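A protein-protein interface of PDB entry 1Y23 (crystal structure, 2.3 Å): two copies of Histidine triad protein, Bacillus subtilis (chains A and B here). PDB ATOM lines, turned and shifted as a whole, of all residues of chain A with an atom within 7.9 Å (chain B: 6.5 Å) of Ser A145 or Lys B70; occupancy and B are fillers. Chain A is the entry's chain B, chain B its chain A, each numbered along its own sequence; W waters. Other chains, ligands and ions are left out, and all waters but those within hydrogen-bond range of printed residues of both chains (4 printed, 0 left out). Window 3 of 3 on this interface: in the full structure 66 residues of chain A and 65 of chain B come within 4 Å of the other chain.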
ATOM      1  N   VAL A  53       4.811 -34.711   5.314  1.00  0.00           N
ATOM      2  CA  VAL A  53       5.957 -34.358   6.129  1.00  0.00           C
ATOM      3  C   VAL A  53       5.660 -34.381   7.633  1.00  0.00           C
ATOM      4  O   VAL A  53       6.572 -34.569   8.438  1.00  0.00           O
ATOM      5  CB  VAL A  53       6.531 -32.976   5.703  1.00  0.00           C
ATOM      6  CG1 VAL A  53       5.626 -31.843   6.168  1.00  0.00           C
ATOM      7  CG2 VAL A  53       7.923 -32.815   6.242  1.00  0.00           C
ATOM      8  N   TYR A  54       4.389 -34.230   8.004  1.00  0.00           N
ATOM      9  CA  TYR A  54       3.972 -34.220   9.411  1.00  0.00           C
ATOM     10  C   TYR A  54       4.160 -35.549  10.145  1.00  0.00           C
ATOM     11  O   TYR A  54       4.428 -35.570  11.352  1.00  0.00           O
ATOM     12  CB  TYR A  54       2.494 -33.824   9.534  1.00  0.00           C
ATOM     13  CG  TYR A  54       2.148 -32.497   8.916  1.00  0.00           C
ATOM     14  CD1 TYR A  54       1.242 -32.415   7.856  1.00  0.00           C
ATOM     15  CD2 TYR A  54       2.731 -31.318   9.380  1.00  0.00           C
ATOM     16  CE1 TYR A  54       0.925 -31.189   7.272  1.00  0.00           C
ATOM     17  CE2 TYR A  54       2.420 -30.090   8.802  1.00  0.00           C
ATOM     18  CZ  TYR A  54       1.518 -30.033   7.748  1.00  0.00           C
ATOM     19  OH  TYR A  54       1.224 -28.829   7.154  1.00  0.00           O
ATOM     20  N   PHE A  56       6.524 -37.642   9.843  1.00  0.00           N
ATOM     21  CA  PHE A  56       7.922 -37.997  10.009  1.00  0.00           C
ATOM     22  C   PHE A  56       8.299 -38.042  11.483  1.00  0.00           C
ATOM     23  O   PHE A  56       7.909 -37.157  12.246  1.00  0.00           O
ATOM     24  CB  PHE A  56       8.832 -36.966   9.320  1.00  0.00           C
ATOM     25  CG  PHE A  56       9.437 -37.443   8.029  1.00  0.00           C
ATOM     26  CD1 PHE A  56       9.060 -36.877   6.813  1.00  0.00           C
ATOM     27  CD2 PHE A  56      10.361 -38.481   8.028  1.00  0.00           C
ATOM     28  CE1 PHE A  56       9.595 -37.346   5.610  1.00  0.00           C
ATOM     29  CE2 PHE A  56      10.904 -38.960   6.837  1.00  0.00           C
ATOM     30  CZ  PHE A  56      10.518 -38.390   5.623  1.00  0.00           C
ATOM     31  N   THR A  57       9.022 -39.091  11.882  1.00  0.00           N
ATOM     32  CA  THR A  57       9.537 -39.214  13.249  1.00  0.00           C
ATOM     33  C   THR A  57      11.034 -38.962  13.046  1.00  0.00           C
ATOM     34  O   THR A  57      11.514 -38.981  11.910  1.00  0.00           O
ATOM     35  CB  THR A  57       9.399 -40.658  13.867  1.00  0.00           C
ATOM     36  OG1 THR A  57      10.096 -41.610  13.047  1.00  0.00           O
ATOM     37  CG2 THR A  57       7.932 -41.070  14.017  1.00  0.00           C
ATOM     38  N   ASP A  58      11.762 -38.733  14.132  1.00  0.00           N
ATOM     39  CA  ASP A  58      13.198 -38.509  14.032  1.00  0.00           C
ATOM     40  C   ASP A  58      13.902 -39.732  13.448  1.00  0.00           C
ATOM     41  O   ASP A  58      14.764 -39.603  12.577  1.00  0.00           O
ATOM     42  CB  ASP A  58      13.795 -38.169  15.404  1.00  0.00           C
ATOM     43  CG  ASP A  58      13.381 -36.784  15.897  1.00  0.00           C
ATOM     44  OD1 ASP A  58      12.856 -35.991  15.089  1.00  0.00           O
ATOM     45  OD2 ASP A  58      13.595 -36.479  17.093  1.00  0.00           O
ATOM     46  N   ILE A 138       4.682 -19.969  17.424  1.00  0.00           N
ATOM     47  CA  ILE A 138       5.080 -21.235  16.827  1.00  0.00           C
ATOM     48  C   ILE A 138       6.085 -21.906  17.728  1.00  0.00           C
ATOM     49  O   ILE A 138       6.025 -23.107  17.958  1.00  0.00           O
ATOM     50  CB  ILE A 138       5.739 -21.051  15.463  1.00  0.00           C
ATOM     51  CG1 ILE A 138       4.817 -20.260  14.535  1.00  0.00           C
ATOM     52  CG2 ILE A 138       6.048 -22.413  14.860  1.00  0.00           C
ATOM     53  CD1 ILE A 138       5.452 -19.935  13.197  1.00  0.00           C
ATOM     54  N   ALA A 139       7.013 -21.109  18.243  1.00  0.00           N
ATOM     55  CA  ALA A 139       8.047 -21.621  19.115  1.00  0.00           C
ATOM     56  C   ALA A 139       7.472 -22.311  20.358  1.00  0.00           C
ATOM     57  O   ALA A 139       7.951 -23.375  20.739  1.00  0.00           O
ATOM     58  CB  ALA A 139       8.990 -20.494  19.518  1.00  0.00           C
ATOM     59  N   LYS A 140       6.457 -21.715  20.985  1.00  0.00           N
ATOM     60  CA  LYS A 140       5.853 -22.303  22.184  1.00  0.00           C
ATOM     61  C   LYS A 140       5.371 -23.738  21.972  1.00  0.00           C
ATOM     62  O   LYS A 140       5.488 -24.574  22.869  1.00  0.00           O
ATOM     63  CB  LYS A 140       4.675 -21.451  22.697  1.00  0.00           C
ATOM     64  CG  LYS A 140       5.091 -20.214  23.514  1.00  0.00           C
ATOM     65  CD  LYS A 140       3.895 -19.463  24.140  1.00  0.00           C
ATOM     66  CE  LYS A 140       2.998 -18.794  23.087  1.00  0.00           C
ATOM     67  NZ  LYS A 140       1.869 -18.021  23.698  1.00  0.00           N
ATOM     68  N   ARG A 141       4.826 -24.013  20.792  1.00  0.00           N
ATOM     69  CA  ARG A 141       4.328 -25.341  20.470  1.00  0.00           C
ATOM     70  C   ARG A 141       5.494 -26.304  20.292  1.00  0.00           C
ATOM     71  O   ARG A 141       5.342 -27.508  20.475  1.00  0.00           O
ATOM     72  CB  ARG A 141       3.500 -25.283  19.191  1.00  0.00           C
ATOM     73  CG  ARG A 141       2.413 -24.220  19.245  1.00  0.00           C
ATOM     74  CD  ARG A 141       1.748 -24.040  17.888  1.00  0.00           C
ATOM     75  NE  ARG A 141       0.518 -24.802  17.780  1.00  0.00           N
ATOM     76  CZ  ARG A 141      -0.638 -24.431  18.320  1.00  0.00           C
ATOM     77  NH1 ARG A 141      -0.731 -23.301  19.003  1.00  0.00           N
ATOM     78  NH2 ARG A 141      -1.709 -25.197  18.185  1.00  0.00           N
ATOM     79  N   LEU A 142       6.657 -25.749  19.955  1.00  0.00           N
ATOM     80  CA  LEU A 142       7.872 -26.517  19.729  1.00  0.00           C
ATOM     81  C   LEU A 142       8.683 -26.850  20.969  1.00  0.00           C
ATOM     82  O   LEU A 142       9.675 -27.573  20.880  1.00  0.00           O
ATOM     83  CB  LEU A 142       8.770 -25.778  18.738  1.00  0.00           C
ATOM     84  CG  LEU A 142       8.259 -25.741  17.300  1.00  0.00           C
ATOM     85  CD1 LEU A 142       9.051 -24.733  16.476  1.00  0.00           C
ATOM     86  CD2 LEU A 142       8.377 -27.141  16.707  1.00  0.00           C
ATOM     87  N   ALA A 143       8.282 -26.325  22.121  1.00  0.00           N
ATOM     88  CA  ALA A 143       9.011 -26.592  23.360  1.00  0.00           C
ATOM     89  C   ALA A 143       8.953 -28.074  23.706  1.00  0.00           C
ATOM     90  O   ALA A 143       9.779 -28.588  24.460  1.00  0.00           O
ATOM     91  CB  ALA A 143       8.413 -25.776  24.509  1.00  0.00           C
ATOM     92  N   SER A 144       7.976 -28.760  23.136  1.00  0.00           N
ATOM     93  CA  SER A 144       7.771 -30.174  23.407  1.00  0.00           C
ATOM     94  C   SER A 144       8.401 -31.109  22.386  1.00  0.00           C
ATOM     95  O   SER A 144       8.392 -32.317  22.588  1.00  0.00           O
ATOM     96  CB  SER A 144       6.278 -30.452  23.424  1.00  0.00           C
ATOM     97  OG  SER A 144       5.771 -30.286  22.112  1.00  0.00           O
ATOM     98  N   SER A 145       8.945 -30.555  21.304  1.00  0.00           N
ATOM     99  CA  SER A 145       9.508 -31.361  20.219  1.00  0.00           C
ATOM    100  C   SER A 145      10.712 -32.242  20.558  1.00  0.00           C
ATOM    101  O   SER A 145      11.357 -32.030  21.601  1.00  0.00           O
ATOM    102  CB  SER A 145       9.857 -30.463  19.021  1.00  0.00           C
ATOM    103  OG  SER A 145      11.005 -29.678  19.284  1.00  0.00           O
ATOM    104  OXT SER A 145      10.998 -33.144  19.741  1.00  0.00           O
ATOM    105  N   TYR B  23      12.542 -21.644  16.143  1.00  0.00           N
ATOM    106  CA  TYR B  23      13.105 -22.873  16.679  1.00  0.00           C
ATOM    107  C   TYR B  23      14.609 -22.789  16.803  1.00  0.00           C
ATOM    108  O   TYR B  23      15.281 -22.170  15.985  1.00  0.00           O
ATOM    109  CB  TYR B  23      12.767 -24.032  15.745  1.00  0.00           C
ATOM    110  CG  TYR B  23      13.373 -25.355  16.147  1.00  0.00           C
ATOM    111  CD1 TYR B  23      12.646 -26.273  16.904  1.00  0.00           C
ATOM    112  CD2 TYR B  23      14.670 -25.703  15.748  1.00  0.00           C
ATOM    113  CE1 TYR B  23      13.186 -27.506  17.247  1.00  0.00           C
ATOM    114  CE2 TYR B  23      15.224 -26.932  16.089  1.00  0.00           C
ATOM    115  CZ  TYR B  23      14.473 -27.834  16.839  1.00  0.00           C
ATOM    116  OH  TYR B  23      14.995 -29.065  17.174  1.00  0.00           O
ATOM    117  N   ASP B  25      18.089 -25.251  18.412  1.00  0.00           N
ATOM    118  CA  ASP B  25      18.677 -26.302  19.199  1.00  0.00           C
ATOM    119  C   ASP B  25      20.163 -26.245  18.948  1.00  0.00           C
ATOM    120  O   ASP B  25      20.703 -25.229  18.480  1.00  0.00           O
ATOM    121  CB  ASP B  25      18.095 -27.687  18.853  1.00  0.00           C
ATOM    122  CG  ASP B  25      18.512 -28.196  17.483  1.00  0.00           C
ATOM    123  OD1 ASP B  25      18.001 -29.256  17.081  1.00  0.00           O
ATOM    124  OD2 ASP B  25      19.341 -27.557  16.807  1.00  0.00           O
ATOM    125  N   PHE B  65      17.588 -32.358   9.277  1.00  0.00           N
ATOM    126  CA  PHE B  65      16.250 -32.677   8.792  1.00  0.00           C
ATOM    127  C   PHE B  65      15.124 -32.921   9.794  1.00  0.00           C
ATOM    128  O   PHE B  65      13.991 -32.497   9.552  1.00  0.00           O
ATOM    129  CB  PHE B  65      16.326 -33.853   7.811  1.00  0.00           C
ATOM    130  CG  PHE B  65      15.055 -34.077   7.033  1.00  0.00           C
ATOM    131  CD1 PHE B  65      14.491 -33.041   6.278  1.00  0.00           C
ATOM    132  CD2 PHE B  65      14.415 -35.316   7.058  1.00  0.00           C
ATOM    133  CE1 PHE B  65      13.306 -33.236   5.563  1.00  0.00           C
ATOM    134  CE2 PHE B  65      13.231 -35.527   6.349  1.00  0.00           C
ATOM    135  CZ  PHE B  65      12.674 -34.482   5.597  1.00  0.00           C
ATOM    136  N   HIS B  66      15.430 -33.583  10.906  1.00  0.00           N
ATOM    137  CA  HIS B  66      14.435 -33.886  11.935  1.00  0.00           C
ATOM    138  C   HIS B  66      13.649 -32.646  12.397  1.00  0.00           C
ATOM    139  O   HIS B  66      12.513 -32.753  12.853  1.00  0.00           O
ATOM    140  CB  HIS B  66      15.122 -34.505  13.156  1.00  0.00           C
ATOM    141  CG  HIS B  66      15.848 -33.503  13.995  1.00  0.00           C
ATOM    142  ND1 HIS B  66      17.084 -32.998  13.647  1.00  0.00           N
ATOM    143  CD2 HIS B  66      15.491 -32.872  15.135  1.00  0.00           C
ATOM    144  CE1 HIS B  66      17.456 -32.098  14.541  1.00  0.00           C
ATOM    145  NE2 HIS B  66      16.505 -32.004  15.457  1.00  0.00           N
ATOM    146  N   ALA B  67      14.269 -31.477  12.285  1.00  0.00           N
ATOM    147  CA  ALA B  67      13.641 -30.228  12.705  1.00  0.00           C
ATOM    148  C   ALA B  67      12.528 -29.757  11.757  1.00  0.00           C
ATOM    149  O   ALA B  67      11.576 -29.115  12.192  1.00  0.00           O
ATOM    150  CB  ALA B  67      14.702 -29.140  12.844  1.00  0.00           C
ATOM    151  N   VAL B  68      12.646 -30.081  10.473  1.00  0.00           N
ATOM    152  CA  VAL B  68      11.658 -29.670   9.485  1.00  0.00           C
ATOM    153  C   VAL B  68      10.265 -30.229   9.778  1.00  0.00           C
ATOM    154  O   VAL B  68       9.280 -29.487   9.739  1.00  0.00           O
ATOM    155  CB  VAL B  68      12.105 -30.079   8.047  1.00  0.00           C
ATOM    156  CG1 VAL B  68      10.995 -29.811   7.045  1.00  0.00           C
ATOM    157  CG2 VAL B  68      13.361 -29.295   7.659  1.00  0.00           C
ATOM    158  N   PRO B  69      10.154 -31.541  10.072  1.00  0.00           N
ATOM    159  CA  PRO B  69       8.814 -32.074  10.354  1.00  0.00           C
ATOM    160  C   PRO B  69       8.261 -31.496  11.651  1.00  0.00           C
ATOM    161  O   PRO B  69       7.049 -31.303  11.788  1.00  0.00           O
ATOM    162  CB  PRO B  69       9.045 -33.583  10.435  1.00  0.00           C
ATOM    163  CG  PRO B  69      10.215 -33.790   9.496  1.00  0.00           C
ATOM    164  CD  PRO B  69      11.120 -32.636   9.892  1.00  0.00           C
ATOM    165  N   LYS B  70       9.148 -31.204  12.599  1.00  0.00           N
ATOM    166  CA  LYS B  70       8.714 -30.639  13.871  1.00  0.00           C
ATOM    167  C   LYS B  70       8.198 -29.213  13.680  1.00  0.00           C
ATOM    168  O   LYS B  70       7.157 -28.838  14.223  1.00  0.00           O
ATOM    169  CB  LYS B  70       9.863 -30.657  14.888  1.00  0.00           C
ATOM    170  CG  LYS B  70      10.228 -32.057  15.361  1.00  0.00           C
ATOM    171  CD  LYS B  70      11.517 -32.068  16.160  1.00  0.00           C
ATOM    172  CE  LYS B  70      11.839 -33.474  16.651  1.00  0.00           C
ATOM    173  NZ  LYS B  70      13.233 -33.601  17.148  1.00  0.00           N
ATOM    174  N   ILE B  71       8.920 -28.427  12.894  1.00  0.00           N
ATOM    175  CA  ILE B  71       8.523 -27.055  12.645  1.00  0.00           C
ATOM    176  C   ILE B  71       7.249 -27.027  11.796  1.00  0.00           C
ATOM    177  O   ILE B  71       6.347 -26.225  12.041  1.00  0.00           O
ATOM    178  CB  ILE B  71       9.679 -26.285  11.974  1.00  0.00           C
ATOM    179  CG1 ILE B  71      10.873 -26.256  12.941  1.00  0.00           C
ATOM    180  CG2 ILE B  71       9.244 -24.852  11.627  1.00  0.00           C
ATOM    181  CD1 ILE B  71      12.172 -25.768  12.346  1.00  0.00           C
ATOM    182  N   ALA B  72       7.175 -27.924  10.817  1.00  0.00           N
ATOM    183  CA  ALA B  72       6.013 -28.026   9.950  1.00  0.00           C
ATOM    184  C   ALA B  72       4.753 -28.268  10.781  1.00  0.00           C
ATOM    185  O   ALA B  72       3.731 -27.607  10.574  1.00  0.00           O
ATOM    186  CB  ALA B  72       6.207 -29.158   8.941  1.00  0.00           C
ATOM    187  N   ARG B  73       4.822 -29.214  11.718  1.00  0.00           N
ATOM    188  CA  ARG B  73       3.676 -29.525  12.580  1.00  0.00           C
ATOM    189  C   ARG B  73       3.280 -28.338  13.469  1.00  0.00           C
ATOM    190  O   ARG B  73       2.098 -28.118  13.716  1.00  0.00           O
ATOM    191  CB  ARG B  73       3.968 -30.752  13.464  1.00  0.00           C
ATOM    192  CG  ARG B  73       3.837 -32.123  12.761  1.00  0.00           C
ATOM    193  CD  ARG B  73       3.751 -33.261  13.794  1.00  0.00           C
ATOM    194  NE  ARG B  73       4.964 -33.372  14.603  1.00  0.00           N
ATOM    195  CZ  ARG B  73       6.072 -34.014  14.224  1.00  0.00           C
ATOM    196  NH1 ARG B  73       6.123 -34.609  13.043  1.00  0.00           N
ATOM    197  NH2 ARG B  73       7.131 -34.073  15.030  1.00  0.00           N
ATOM    198  N   ALA B  74       4.274 -27.592  13.953  1.00  0.00           N
ATOM    199  CA  ALA B  74       4.020 -26.428  14.800  1.00  0.00           C
ATOM    200  C   ALA B  74       3.288 -25.345  14.000  1.00  0.00           C
ATOM    201  O   ALA B  74       2.352 -24.718  14.492  1.00  0.00           O
ATOM    202  CB  ALA B  74       5.330 -25.884  15.360  1.00  0.00           C
ATOM    203  N   ILE B  75       3.717 -25.138  12.762  1.00  0.00           N
ATOM    204  CA  ILE B  75       3.093 -24.153  11.900  1.00  0.00           C
ATOM    205  C   ILE B  75       1.698 -24.661  11.509  1.00  0.00           C
ATOM    206  O   ILE B  75       0.766 -23.877  11.293  1.00  0.00           O
ATOM    207  CB  ILE B  75       3.978 -23.894  10.646  1.00  0.00           C
ATOM    208  CG1 ILE B  75       5.237 -23.131  11.079  1.00  0.00           C
ATOM    209  CG2 ILE B  75       3.197 -23.119   9.580  1.00  0.00           C
ATOM    210  CD1 ILE B  75       6.326 -23.050  10.062  1.00  0.00           C
HETATM  211  O   HOH W   1      13.717 -31.002  19.183  1.00  0.00           O
HETATM  212  O   HOH W   2      11.570 -35.361  13.048  1.00  0.00           O
HETATM  213  O   HOH W   3       9.200 -35.754  14.220  1.00  0.00           O
HETATM  214  O   HOH W   4      13.233 -34.474  20.092  1.00  0.00           O
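OD2 of Asp A58 lies within salt-bridge range of NZ of Lys B70 (2.9 Å).
OXT of Ser A145 is in salt-bridge range of NZ of Lys B70 (3.5 Å).
The backbone carbonyl oxygen (O) of Tyr A54 sits at hydrogen-bond distance from the guanidinium group (NH1) of Arg B73, at 2.6 Å.
NH1 of Arg B73 lies within hydrogen-bond range of O of Phe A56, at 3.2 Å.
Of chain B, only Tyr B23 and Lys B70 come within 4 Å of Ser A145.
Lys B70 touches just these residues of chain A: Asp A58, Leu A142 and Ser A145.
Of the printed residues of chain A, His B66 touches Asp A58.
Of the printed residues of chain B, Asp A58 touches His B66 (3.3 Å) and Lys B70 (2.9 Å).
Of the printed residues of chain A, Tyr B23 touches Leu A142 (3.9 Å) and Ser A145 (3.7 Å).
Printed residues of chain A within 4 Å of Ala B74: Ile A138 (3.6 Å), Arg A141 (3.5 Å) and Leu A142 (3.5 Å).
Of the printed residues of chain B, Tyr A54 touches Ala B72 (3.3 Å) and Arg B73 (2.6 Å).
Lys A140 touches none of the printed residues of chain B.
The nearest residue of chain A that does not touch Lys B70 is Val A53 (5.9 Å).
The nearest printed residue of chain B that does not touch Val A53 is Val B68 (4.4 Å).
The side-chain hydroxyl (OH) of Tyr B23 is in hydrogen-bond range of the side-chain carboxylate (OD1) of Asp B25 (3.0 Å).
The backbone carbonyl oxygen of Leu A142 is in hydrogen-bond range of the side-chain hydroxyl of Ser A145 (3.0 Å).
Among the printed residues, pairs that only touch across the chains: Val A53 with Pro B69, Val A53 with Ala B72, Tyr A54 with Ala B72, Phe A56 with Pro B69, Asp A58 with His B66, Ile A138 with Ala B74, Ile A138 with Ile B75, Arg A141 with Ala B74, Leu A142 with Tyr B23, Leu A142 with Lys B70, Leu A142 with Ala B74 and Ser A145 with Tyr B23.
No position is printed for both chains.
Of the 16 pairs that touch across the chains among the printed residues, none has its exchanged pair printed and touching as well.
Water W2 lies within hydrogen-bond range of the side-chain carboxylate (OD1) of Asp A58 and the backbone carbonyl oxygen (O) of His B66.
Water W4 lies within hydrogen-bond range of OXT of Ser A145 (2.6 Å) and NZ of Lys B70 (3.1 Å).
Water W3 bridges O of Phe A56 (2.7 Å) and NH2 of Arg B73 (2.8 Å).
Water W1 lies within hydrogen-bond range of OG of Ser A145 (3.0 Å), OH of Tyr B23 (3.1 Å) and NZ of Lys B70 (3.3 Å).
Of the 13 printed residues of chain B, 8 touch a printed residue of chain A.
Printed residues of chain B that touch a printed residue of chain A: Tyr B23, His B66, Pro B69, Lys B70, Ala B72, Arg B73, Ala B74 and Ile B75.
Hydrophobic or aromatic side chains of chain B within 4 Å of the printed part of chain A: Tyr B23, His B66, Pro B69, Ala B72, Ala B74 and Ile B75.
Printed residues of chain A that touch a printed residue of chain B: Val A53, Tyr A54, Phe A56, Asp A58, Ile A138, Arg A141, Leu A142 and Ser A145.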
